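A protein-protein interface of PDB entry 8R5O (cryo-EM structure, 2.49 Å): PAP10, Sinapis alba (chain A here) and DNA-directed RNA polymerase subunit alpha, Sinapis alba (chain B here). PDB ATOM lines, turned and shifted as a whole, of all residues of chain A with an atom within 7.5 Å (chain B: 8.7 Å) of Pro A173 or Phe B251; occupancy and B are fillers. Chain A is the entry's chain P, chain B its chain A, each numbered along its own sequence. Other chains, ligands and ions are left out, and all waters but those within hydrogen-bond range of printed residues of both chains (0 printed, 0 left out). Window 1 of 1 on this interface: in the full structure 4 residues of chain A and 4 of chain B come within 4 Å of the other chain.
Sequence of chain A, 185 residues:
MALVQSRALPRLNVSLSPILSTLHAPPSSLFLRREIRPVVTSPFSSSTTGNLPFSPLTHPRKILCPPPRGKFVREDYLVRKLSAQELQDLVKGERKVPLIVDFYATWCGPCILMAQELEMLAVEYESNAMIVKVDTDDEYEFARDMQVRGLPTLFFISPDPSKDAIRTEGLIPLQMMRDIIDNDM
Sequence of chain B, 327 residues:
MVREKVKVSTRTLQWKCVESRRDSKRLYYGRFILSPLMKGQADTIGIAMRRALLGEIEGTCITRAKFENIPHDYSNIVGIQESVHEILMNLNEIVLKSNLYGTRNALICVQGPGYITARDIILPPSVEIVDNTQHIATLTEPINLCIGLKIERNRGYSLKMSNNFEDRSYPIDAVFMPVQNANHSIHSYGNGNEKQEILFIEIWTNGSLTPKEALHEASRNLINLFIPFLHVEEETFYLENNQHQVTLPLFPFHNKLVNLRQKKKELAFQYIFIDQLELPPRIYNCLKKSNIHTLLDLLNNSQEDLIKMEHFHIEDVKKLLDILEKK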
ATOM      1  N   LEU A 113     -21.014   7.293 -31.147  1.00  0.00           N
ATOM      2  CA  LEU A 113     -19.755   7.126 -30.424  1.00  0.00           C
ATOM      3  C   LEU A 113     -18.592   6.909 -31.384  1.00  0.00           C
ATOM      4  O   LEU A 113     -17.486   7.407 -31.150  1.00  0.00           O
ATOM      5  CB  LEU A 113     -19.858   5.956 -29.447  1.00  0.00           C
ATOM      6  CG  LEU A 113     -20.715   6.138 -28.198  1.00  0.00           C
ATOM      7  CD1 LEU A 113     -20.936   4.801 -27.514  1.00  0.00           C
ATOM      8  CD2 LEU A 113     -20.060   7.122 -27.249  1.00  0.00           C
ATOM      9  N   MET A 114     -18.823   6.154 -32.459  1.00  0.00           N
ATOM     10  CA  MET A 114     -17.784   5.944 -33.461  1.00  0.00           C
ATOM     11  C   MET A 114     -17.397   7.250 -34.143  1.00  0.00           C
ATOM     12  O   MET A 114     -16.233   7.437 -34.513  1.00  0.00           O
ATOM     13  CB  MET A 114     -18.259   4.916 -34.491  1.00  0.00           C
ATOM     14  CG  MET A 114     -17.329   4.716 -35.678  1.00  0.00           C
ATOM     15  SD  MET A 114     -15.734   3.997 -35.243  1.00  0.00           S
ATOM     16  CE  MET A 114     -16.209   2.320 -34.824  1.00  0.00           C
ATOM     17  N   GLU A 117     -14.723   8.965 -32.050  1.00  0.00           N
ATOM     18  CA  GLU A 117     -13.400   8.369 -32.215  1.00  0.00           C
ATOM     19  C   GLU A 117     -12.772   8.773 -33.543  1.00  0.00           C
ATOM     20  O   GLU A 117     -11.574   9.063 -33.608  1.00  0.00           O
ATOM     21  CB  GLU A 117     -13.484   6.846 -32.118  1.00  0.00           C
ATOM     22  CG  GLU A 117     -13.742   6.316 -30.721  1.00  0.00           C
ATOM     23  CD  GLU A 117     -13.727   4.802 -30.658  1.00  0.00           C
ATOM     24  OE1 GLU A 117     -14.259   4.158 -31.584  1.00  0.00           O
ATOM     25  OE2 GLU A 117     -13.175   4.253 -29.683  1.00  0.00           O
ATOM     26  N   LEU A 154     -16.449  -0.108 -40.529  1.00  0.00           N
ATOM     27  CA  LEU A 154     -15.390   0.692 -41.125  1.00  0.00           C
ATOM     28  C   LEU A 154     -14.695  -0.103 -42.219  1.00  0.00           C
ATOM     29  O   LEU A 154     -14.480  -1.311 -42.081  1.00  0.00           O
ATOM     30  CB  LEU A 154     -14.362   1.133 -40.080  1.00  0.00           C
ATOM     31  CG  LEU A 154     -14.883   1.830 -38.823  1.00  0.00           C
ATOM     32  CD1 LEU A 154     -13.725   2.235 -37.934  1.00  0.00           C
ATOM     33  CD2 LEU A 154     -15.732   3.033 -39.184  1.00  0.00           C
ATOM     34  N   GLY A 170     -18.322  -3.247 -35.334  1.00  0.00           N
ATOM     35  CA  GLY A 170     -18.458  -2.890 -33.940  1.00  0.00           C
ATOM     36  C   GLY A 170     -17.628  -1.683 -33.561  1.00  0.00           C
ATOM     37  O   GLY A 170     -16.921  -1.076 -34.369  1.00  0.00           O
ATOM     38  N   LEU A 171     -17.721  -1.330 -32.283  1.00  0.00           N
ATOM     39  CA  LEU A 171     -17.012  -0.176 -31.737  1.00  0.00           C
ATOM     40  C   LEU A 171     -15.625  -0.639 -31.306  1.00  0.00           C
ATOM     41  O   LEU A 171     -15.453  -1.206 -30.225  1.00  0.00           O
ATOM     42  CB  LEU A 171     -17.797   0.430 -30.579  1.00  0.00           C
ATOM     43  CG  LEU A 171     -17.519   1.874 -30.172  1.00  0.00           C
ATOM     44  CD1 LEU A 171     -17.493   2.787 -31.386  1.00  0.00           C
ATOM     45  CD2 LEU A 171     -18.584   2.330 -29.193  1.00  0.00           C
ATOM     46  N   ILE A 172     -14.631  -0.396 -32.154  1.00  0.00           N
ATOM     47  CA  ILE A 172     -13.266  -0.850 -31.898  1.00  0.00           C
ATOM     48  C   ILE A 172     -12.462   0.291 -31.285  1.00  0.00           C
ATOM     49  O   ILE A 172     -12.726   1.463 -31.580  1.00  0.00           O
ATOM     50  CB  ILE A 172     -12.603  -1.371 -33.184  1.00  0.00           C
ATOM     51  CG1 ILE A 172     -12.667  -0.315 -34.290  1.00  0.00           C
ATOM     52  CG2 ILE A 172     -13.253  -2.673 -33.626  1.00  0.00           C
ATOM     53  CD1 ILE A 172     -11.908  -0.688 -35.545  1.00  0.00           C
ATOM     54  N   PRO A 173     -11.487   0.000 -30.425  1.00  0.00           N
ATOM     55  CA  PRO A 173     -10.702   1.071 -29.805  1.00  0.00           C
ATOM     56  C   PRO A 173      -9.812   1.786 -30.812  1.00  0.00           C
ATOM     57  O   PRO A 173      -9.518   1.287 -31.900  1.00  0.00           O
ATOM     58  CB  PRO A 173      -9.869   0.337 -28.750  1.00  0.00           C
ATOM     59  CG  PRO A 173      -9.828  -1.076 -29.212  1.00  0.00           C
ATOM     60  CD  PRO A 173     -11.133  -1.325 -29.894  1.00  0.00           C
ATOM     61  N   LEU A 174      -9.390   2.992 -30.420  1.00  0.00           N
ATOM     62  CA  LEU A 174      -8.593   3.837 -31.305  1.00  0.00           C
ATOM     63  C   LEU A 174      -7.281   3.167 -31.691  1.00  0.00           C
ATOM     64  O   LEU A 174      -6.832   3.285 -32.834  1.00  0.00           O
ATOM     65  CB  LEU A 174      -8.315   5.179 -30.634  1.00  0.00           C
ATOM     66  CG  LEU A 174      -8.812   6.449 -31.319  1.00  0.00           C
ATOM     67  CD1 LEU A 174      -8.289   7.660 -30.576  1.00  0.00           C
ATOM     68  CD2 LEU A 174      -8.394   6.492 -32.779  1.00  0.00           C
ATOM     69  N   GLN A 175      -6.648   2.472 -30.743  1.00  0.00           N
ATOM     70  CA  GLN A 175      -5.347   1.866 -31.005  1.00  0.00           C
ATOM     71  C   GLN A 175      -5.412   0.847 -32.134  1.00  0.00           C
ATOM     72  O   GLN A 175      -4.447   0.706 -32.893  1.00  0.00           O
ATOM     73  CB  GLN A 175      -4.806   1.219 -29.730  1.00  0.00           C
ATOM     74  CG  GLN A 175      -3.413   0.629 -29.873  1.00  0.00           C
ATOM     75  CD  GLN A 175      -2.381   1.656 -30.295  1.00  0.00           C
ATOM     76  OE1 GLN A 175      -2.418   2.808 -29.863  1.00  0.00           O
ATOM     77  NE2 GLN A 175      -1.453   1.244 -31.151  1.00  0.00           N
ATOM     78  N   MET A 176      -6.530   0.132 -32.266  1.00  0.00           N
ATOM     79  CA  MET A 176      -6.657  -0.817 -33.367  1.00  0.00           C
ATOM     80  C   MET A 176      -6.674  -0.103 -34.712  1.00  0.00           C
ATOM     81  O   MET A 176      -6.079  -0.586 -35.682  1.00  0.00           O
ATOM     82  CB  MET A 176      -7.913  -1.668 -33.199  1.00  0.00           C
ATOM     83  CG  MET A 176      -8.017  -2.788 -34.222  1.00  0.00           C
ATOM     84  SD  MET A 176      -9.616  -3.608 -34.223  1.00  0.00           S
ATOM     85  CE  MET A 176      -9.903  -3.735 -32.467  1.00  0.00           C
ATOM     86  N   MET A 177      -7.349   1.047 -34.792  1.00  0.00           N
ATOM     87  CA  MET A 177      -7.339   1.823 -36.028  1.00  0.00           C
ATOM     88  C   MET A 177      -5.931   2.293 -36.371  1.00  0.00           C
ATOM     89  O   MET A 177      -5.525   2.259 -37.537  1.00  0.00           O
ATOM     90  CB  MET A 177      -8.280   3.021 -35.912  1.00  0.00           C
ATOM     91  CG  MET A 177      -9.719   2.669 -35.600  1.00  0.00           C
ATOM     92  SD  MET A 177     -10.748   4.144 -35.507  1.00  0.00           S
ATOM     93  CE  MET A 177     -12.231   3.472 -34.778  1.00  0.00           C
ATOM     94  N   ARG A 178      -5.178   2.744 -35.368  1.00  0.00           N
ATOM     95  CA  ARG A 178      -3.796   3.142 -35.605  1.00  0.00           C
ATOM     96  C   ARG A 178      -2.955   1.959 -36.068  1.00  0.00           C
ATOM     97  O   ARG A 178      -2.100   2.103 -36.950  1.00  0.00           O
ATOM     98  CB  ARG A 178      -3.203   3.763 -34.339  1.00  0.00           C
ATOM     99  CG  ARG A 178      -3.908   5.030 -33.888  1.00  0.00           C
ATOM    100  CD  ARG A 178      -3.090   5.784 -32.852  1.00  0.00           C
ATOM    101  NE  ARG A 178      -3.322   5.308 -31.493  1.00  0.00           N
ATOM    102  CZ  ARG A 178      -3.963   5.998 -30.560  1.00  0.00           C
ATOM    103  NH1 ARG A 178      -4.441   7.207 -30.800  1.00  0.00           N
ATOM    104  NH2 ARG A 178      -4.124   5.462 -29.352  1.00  0.00           N
ATOM    105  N   ASP A 179      -3.180   0.781 -35.483  1.00  0.00           N
ATOM    106  CA  ASP A 179      -2.455  -0.409 -35.915  1.00  0.00           C
ATOM    107  C   ASP A 179      -2.804  -0.786 -37.349  1.00  0.00           C
ATOM    108  O   ASP A 179      -1.918  -1.141 -38.134  1.00  0.00           O
ATOM    109  CB  ASP A 179      -2.744  -1.574 -34.970  1.00  0.00           C
ATOM    110  CG  ASP A 179      -2.255  -1.317 -33.562  1.00  0.00           C
ATOM    111  OD1 ASP A 179      -1.637  -0.256 -33.329  1.00  0.00           O
ATOM    112  OD2 ASP A 179      -2.490  -2.176 -32.685  1.00  0.00           O
ATOM    113  N   PHE B 237     -15.266  -3.801 -12.933  1.00  0.00           N
ATOM    114  CA  PHE B 237     -14.429  -3.702 -14.117  1.00  0.00           C
ATOM    115  C   PHE B 237     -13.162  -2.922 -13.799  1.00  0.00           C
ATOM    116  O   PHE B 237     -13.144  -2.054 -12.922  1.00  0.00           O
ATOM    117  CB  PHE B 237     -15.179  -3.026 -15.264  1.00  0.00           C
ATOM    118  CG  PHE B 237     -16.448  -3.723 -15.652  1.00  0.00           C
ATOM    119  CD1 PHE B 237     -16.415  -4.996 -16.192  1.00  0.00           C
ATOM    120  CD2 PHE B 237     -17.672  -3.101 -15.489  1.00  0.00           C
ATOM    121  CE1 PHE B 237     -17.583  -5.640 -16.553  1.00  0.00           C
ATOM    122  CE2 PHE B 237     -18.841  -3.739 -15.851  1.00  0.00           C
ATOM    123  CZ  PHE B 237     -18.797  -5.010 -16.381  1.00  0.00           C
ATOM    124  N   TYR B 238     -12.094  -3.250 -14.521  1.00  0.00           N
ATOM    125  CA  TYR B 238     -10.816  -2.583 -14.323  1.00  0.00           C
ATOM    126  C   TYR B 238     -10.915  -1.107 -14.690  1.00  0.00           C
ATOM    127  O   TYR B 238     -11.485  -0.746 -15.723  1.00  0.00           O
ATOM    128  CB  TYR B 238      -9.735  -3.269 -15.157  1.00  0.00           C
ATOM    129  CG  TYR B 238      -8.459  -2.468 -15.289  1.00  0.00           C
ATOM    130  CD1 TYR B 238      -7.484  -2.514 -14.305  1.00  0.00           C
ATOM    131  CD2 TYR B 238      -8.231  -1.666 -16.398  1.00  0.00           C
ATOM    132  CE1 TYR B 238      -6.319  -1.782 -14.420  1.00  0.00           C
ATOM    133  CE2 TYR B 238      -7.071  -0.930 -16.522  1.00  0.00           C
ATOM    134  CZ  TYR B 238      -6.118  -0.993 -15.528  1.00  0.00           C
ATOM    135  OH  TYR B 238      -4.958  -0.263 -15.647  1.00  0.00           O
ATOM    136  N   LEU B 239     -10.346  -0.255 -13.843  1.00  0.00           N
ATOM    137  CA  LEU B 239     -10.318   1.182 -14.095  1.00  0.00           C
ATOM    138  C   LEU B 239      -8.884   1.693 -14.145  1.00  0.00           C
ATOM    139  O   LEU B 239      -8.017   1.201 -13.422  1.00  0.00           O
ATOM    140  CB  LEU B 239     -11.109   1.931 -13.022  1.00  0.00           C
ATOM    141  CG  LEU B 239     -12.631   1.807 -13.101  1.00  0.00           C
ATOM    142  CD1 LEU B 239     -13.284   2.368 -11.849  1.00  0.00           C
ATOM    143  CD2 LEU B 239     -13.148   2.512 -14.340  1.00  0.00           C
ATOM    144  N   THR B 247     -17.997   5.237 -19.624  1.00  0.00           N
ATOM    145  CA  THR B 247     -18.883   5.226 -20.783  1.00  0.00           C
ATOM    146  C   THR B 247     -18.847   3.866 -21.472  1.00  0.00           C
ATOM    147  O   THR B 247     -19.885   3.284 -21.773  1.00  0.00           O
ATOM    148  CB  THR B 247     -18.507   6.327 -21.796  1.00  0.00           C
ATOM    149  OG1 THR B 247     -18.450   7.592 -21.128  1.00  0.00           O
ATOM    150  CG2 THR B 247     -19.535   6.406 -22.914  1.00  0.00           C
ATOM    151  N   LEU B 248     -17.635   3.367 -21.716  1.00  0.00           N
ATOM    152  CA  LEU B 248     -17.417   2.064 -22.345  1.00  0.00           C
ATOM    153  C   LEU B 248     -16.455   1.283 -21.461  1.00  0.00           C
ATOM    154  O   LEU B 248     -15.231   1.389 -21.611  1.00  0.00           O
ATOM    155  CB  LEU B 248     -16.878   2.218 -23.765  1.00  0.00           C
ATOM    156  CG  LEU B 248     -17.764   3.022 -24.719  1.00  0.00           C
ATOM    157  CD1 LEU B 248     -16.992   3.402 -25.962  1.00  0.00           C
ATOM    158  CD2 LEU B 248     -19.016   2.243 -25.085  1.00  0.00           C
ATOM    159  N   PRO B 249     -16.975   0.481 -20.527  1.00  0.00           N
ATOM    160  CA  PRO B 249     -16.097  -0.180 -19.548  1.00  0.00           C
ATOM    161  C   PRO B 249     -15.136  -1.194 -20.147  1.00  0.00           C
ATOM    162  O   PRO B 249     -14.241  -1.663 -19.432  1.00  0.00           O
ATOM    163  CB  PRO B 249     -17.087  -0.853 -18.586  1.00  0.00           C
ATOM    164  CG  PRO B 249     -18.336  -1.014 -19.381  1.00  0.00           C
ATOM    165  CD  PRO B 249     -18.396   0.172 -20.298  1.00  0.00           C
ATOM    166  N   LEU B 250     -15.288  -1.551 -21.422  1.00  0.00           N
ATOM    167  CA  LEU B 250     -14.376  -2.499 -22.053  1.00  0.00           C
ATOM    168  C   LEU B 250     -13.020  -1.877 -22.372  1.00  0.00           C
ATOM    169  O   LEU B 250     -11.989  -2.544 -22.234  1.00  0.00           O
ATOM    170  CB  LEU B 250     -15.011  -3.055 -23.328  1.00  0.00           C
ATOM    171  CG  LEU B 250     -14.186  -4.037 -24.160  1.00  0.00           C
ATOM    172  CD1 LEU B 250     -13.755  -5.215 -23.314  1.00  0.00           C
ATOM    173  CD2 LEU B 250     -14.974  -4.509 -25.364  1.00  0.00           C
ATOM    174  N   PHE B 251     -13.002  -0.615 -22.790  1.00  0.00           N
ATOM    175  CA  PHE B 251     -11.813   0.059 -23.301  1.00  0.00           C
ATOM    176  C   PHE B 251     -10.655   0.185 -22.307  1.00  0.00           C
ATOM    177  O   PHE B 251      -9.505  -0.033 -22.706  1.00  0.00           O
ATOM    178  CB  PHE B 251     -12.191   1.444 -23.833  1.00  0.00           C
ATOM    179  CG  PHE B 251     -12.821   1.417 -25.197  1.00  0.00           C
ATOM    180  CD1 PHE B 251     -12.990   0.220 -25.872  1.00  0.00           C
ATOM    181  CD2 PHE B 251     -13.229   2.586 -25.809  1.00  0.00           C
ATOM    182  CE1 PHE B 251     -13.562   0.192 -27.128  1.00  0.00           C
ATOM    183  CE2 PHE B 251     -13.800   2.564 -27.066  1.00  0.00           C
ATOM    184  CZ  PHE B 251     -13.969   1.365 -27.725  1.00  0.00           C
ATOM    185  N   PRO B 252     -10.882   0.556 -21.037  1.00  0.00           N
ATOM    186  CA  PRO B 252      -9.729   0.706 -20.127  1.00  0.00           C
ATOM    187  C   PRO B 252      -8.885  -0.549 -19.978  1.00  0.00           C
ATOM    188  O   PRO B 252      -7.658  -0.446 -19.859  1.00  0.00           O
ATOM    189  CB  PRO B 252     -10.381   1.117 -18.796  1.00  0.00           C
ATOM    190  CG  PRO B 252     -11.823   0.776 -18.937  1.00  0.00           C
ATOM    191  CD  PRO B 252     -12.131   0.978 -20.381  1.00  0.00           C
ATOM    192  N   PHE B 253      -9.498  -1.736 -19.978  1.00  0.00           N
ATOM    193  CA  PHE B 253      -8.703  -2.958 -19.908  1.00  0.00           C
ATOM    194  C   PHE B 253      -7.907  -3.183 -21.186  1.00  0.00           C
ATOM    195  O   PHE B 253      -6.798  -3.727 -21.133  1.00  0.00           O
ATOM    196  CB  PHE B 253      -9.591  -4.166 -19.624  1.00  0.00           C
ATOM    197  CG  PHE B 253      -8.825  -5.444 -19.412  1.00  0.00           C
ATOM    198  CD1 PHE B 253      -8.280  -5.741 -18.174  1.00  0.00           C
ATOM    199  CD2 PHE B 253      -8.649  -6.345 -20.447  1.00  0.00           C
ATOM    200  CE1 PHE B 253      -7.576  -6.911 -17.975  1.00  0.00           C
ATOM    201  CE2 PHE B 253      -7.945  -7.515 -20.255  1.00  0.00           C
ATOM    202  CZ  PHE B 253      -7.409  -7.800 -19.016  1.00  0.00           C
ATOM    203  N   HIS B 254      -8.456  -2.795 -22.338  1.00  0.00           N
ATOM    204  CA  HIS B 254      -7.710  -2.909 -23.588  1.00  0.00           C
ATOM    205  C   HIS B 254      -6.454  -2.051 -23.555  1.00  0.00           C
ATOM    206  O   HIS B 254      -5.379  -2.485 -23.984  1.00  0.00           O
ATOM    207  CB  HIS B 254      -8.591  -2.517 -24.771  1.00  0.00           C
ATOM    208  CG  HIS B 254      -7.836  -2.386 -26.057  1.00  0.00           C
ATOM    209  ND1 HIS B 254      -7.568  -3.462 -26.875  1.00  0.00           N
ATOM    210  CD2 HIS B 254      -7.277  -1.309 -26.658  1.00  0.00           C
ATOM    211  CE1 HIS B 254      -6.885  -3.053 -27.928  1.00  0.00           C
ATOM    212  NE2 HIS B 254      -6.694  -1.751 -27.820  1.00  0.00           N
ATOM    213  N   ASN B 255      -6.574  -0.817 -23.059  1.00  0.00           N
ATOM    214  CA  ASN B 255      -5.412   0.059 -22.958  1.00  0.00           C
ATOM    215  C   ASN B 255      -4.364  -0.512 -22.013  1.00  0.00           C
ATOM    216  O   ASN B 255      -3.166  -0.277 -22.202  1.00  0.00           O
ATOM    217  CB  ASN B 255      -5.844   1.450 -22.496  1.00  0.00           C
ATOM    218  CG  ASN B 255      -4.701   2.442 -22.491  1.00  0.00           C
ATOM    219  OD1 ASN B 255      -3.810   2.383 -23.338  1.00  0.00           O
ATOM    220  ND2 ASN B 255      -4.717   3.357 -21.532  1.00  0.00           N
ATOM    221  N   LYS B 256      -4.795  -1.255 -20.992  1.00  0.00           N
ATOM    222  CA  LYS B 256      -3.847  -1.948 -20.126  1.00  0.00           C
ATOM    223  C   LYS B 256      -3.058  -2.994 -20.901  1.00  0.00           C
ATOM    224  O   LYS B 256      -1.852  -3.161 -20.681  1.00  0.00           O
ATOM    225  CB  LYS B 256      -4.590  -2.589 -18.955  1.00  0.00           C
ATOM    226  CG  LYS B 256      -3.721  -3.421 -18.033  1.00  0.00           C
ATOM    227  CD  LYS B 256      -4.571  -4.223 -17.062  1.00  0.00           C
ATOM    228  CE  LYS B 256      -3.712  -4.932 -16.034  1.00  0.00           C
ATOM    229  NZ  LYS B 256      -2.981  -3.968 -15.169  1.00  0.00           N
ATOM    230  N   LEU B 257      -3.722  -3.713 -21.810  1.00  0.00           N
ATOM    231  CA  LEU B 257      -3.039  -4.733 -22.603  1.00  0.00           C
ATOM    232  C   LEU B 257      -2.031  -4.113 -23.564  1.00  0.00           C
ATOM    233  O   LEU B 257      -0.949  -4.671 -23.777  1.00  0.00           O
ATOM    234  CB  LEU B 257      -4.062  -5.573 -23.365  1.00  0.00           C
ATOM    235  CG  LEU B 257      -5.005  -6.431 -22.520  1.00  0.00           C
ATOM    236  CD1 LEU B 257      -6.151  -6.948 -23.364  1.00  0.00           C
ATOM    237  CD2 LEU B 257      -4.250  -7.585 -21.887  1.00  0.00           C
ATOM    238  N   VAL B 258      -2.375  -2.973 -24.167  1.00  0.00           N
ATOM    239  CA  VAL B 258      -1.424  -2.277 -25.029  1.00  0.00           C
ATOM    240  C   VAL B 258      -0.193  -1.866 -24.233  1.00  0.00           C
ATOM    241  O   VAL B 258       0.944  -2.009 -24.698  1.00  0.00           O
ATOM    242  CB  VAL B 258      -2.095  -1.064 -25.704  1.00  0.00           C
ATOM    243  CG1 VAL B 258      -1.092  -0.308 -26.561  1.00  0.00           C
ATOM    244  CG2 VAL B 258      -3.287  -1.512 -26.539  1.00  0.00           C
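Printed residues of chain A within 4 Å of Phe B251: Glu A117 (3.2 Å), Leu A171 (3.9 Å) and Pro A173 (3.9 Å). Printed residues of chain A within 4 Å of Leu B248: Leu A171 (3.8 Å). Of the printed residues of chain A, Val B258 touches Gln A175. Of the printed residues of chain B, Leu A171 touches Leu B248 (3.8 Å) and Phe B251 (3.9 Å). Printed residues of chain B within 4 Å of Glu A117: Phe B251 (3.2 Å). Of the printed residues of chain A, His B254 touches Pro A173. The nearest residue of chain B that does not touch Pro A173 is Asn B255 (6.7 Å). The nearest printed residue of chain A that does not touch Phe B251 is Ile A172 (4.01 Å). The nearest printed residue of chain A that does not touch Leu B248 is Leu A113 (4.02 Å).
Among the printed residues, merely in contact across the chains: Glu A117 with Phe B251 (3.2 Å), Leu A171 with Leu B248 (3.8 Å), Leu A171 with Phe B251 (3.9 Å), Pro A173 with Phe B251 (3.9 Å), Pro A173 with His B254 (3.5 Å) and Gln A175 with Val B258 (3.96 Å).
OE1 of Gln A175 is in hydrogen-bond range of NE of Arg A178 (3.1 Å). The side-chain amide nitrogen (NE2) of Gln A175 is in hydrogen-bond range of the side-chain carboxylate (OD1) of Asp A179.
Printed residues of chain B that touch a printed residue of chain A: Leu B248, Phe B251, His B254 and Val B258.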
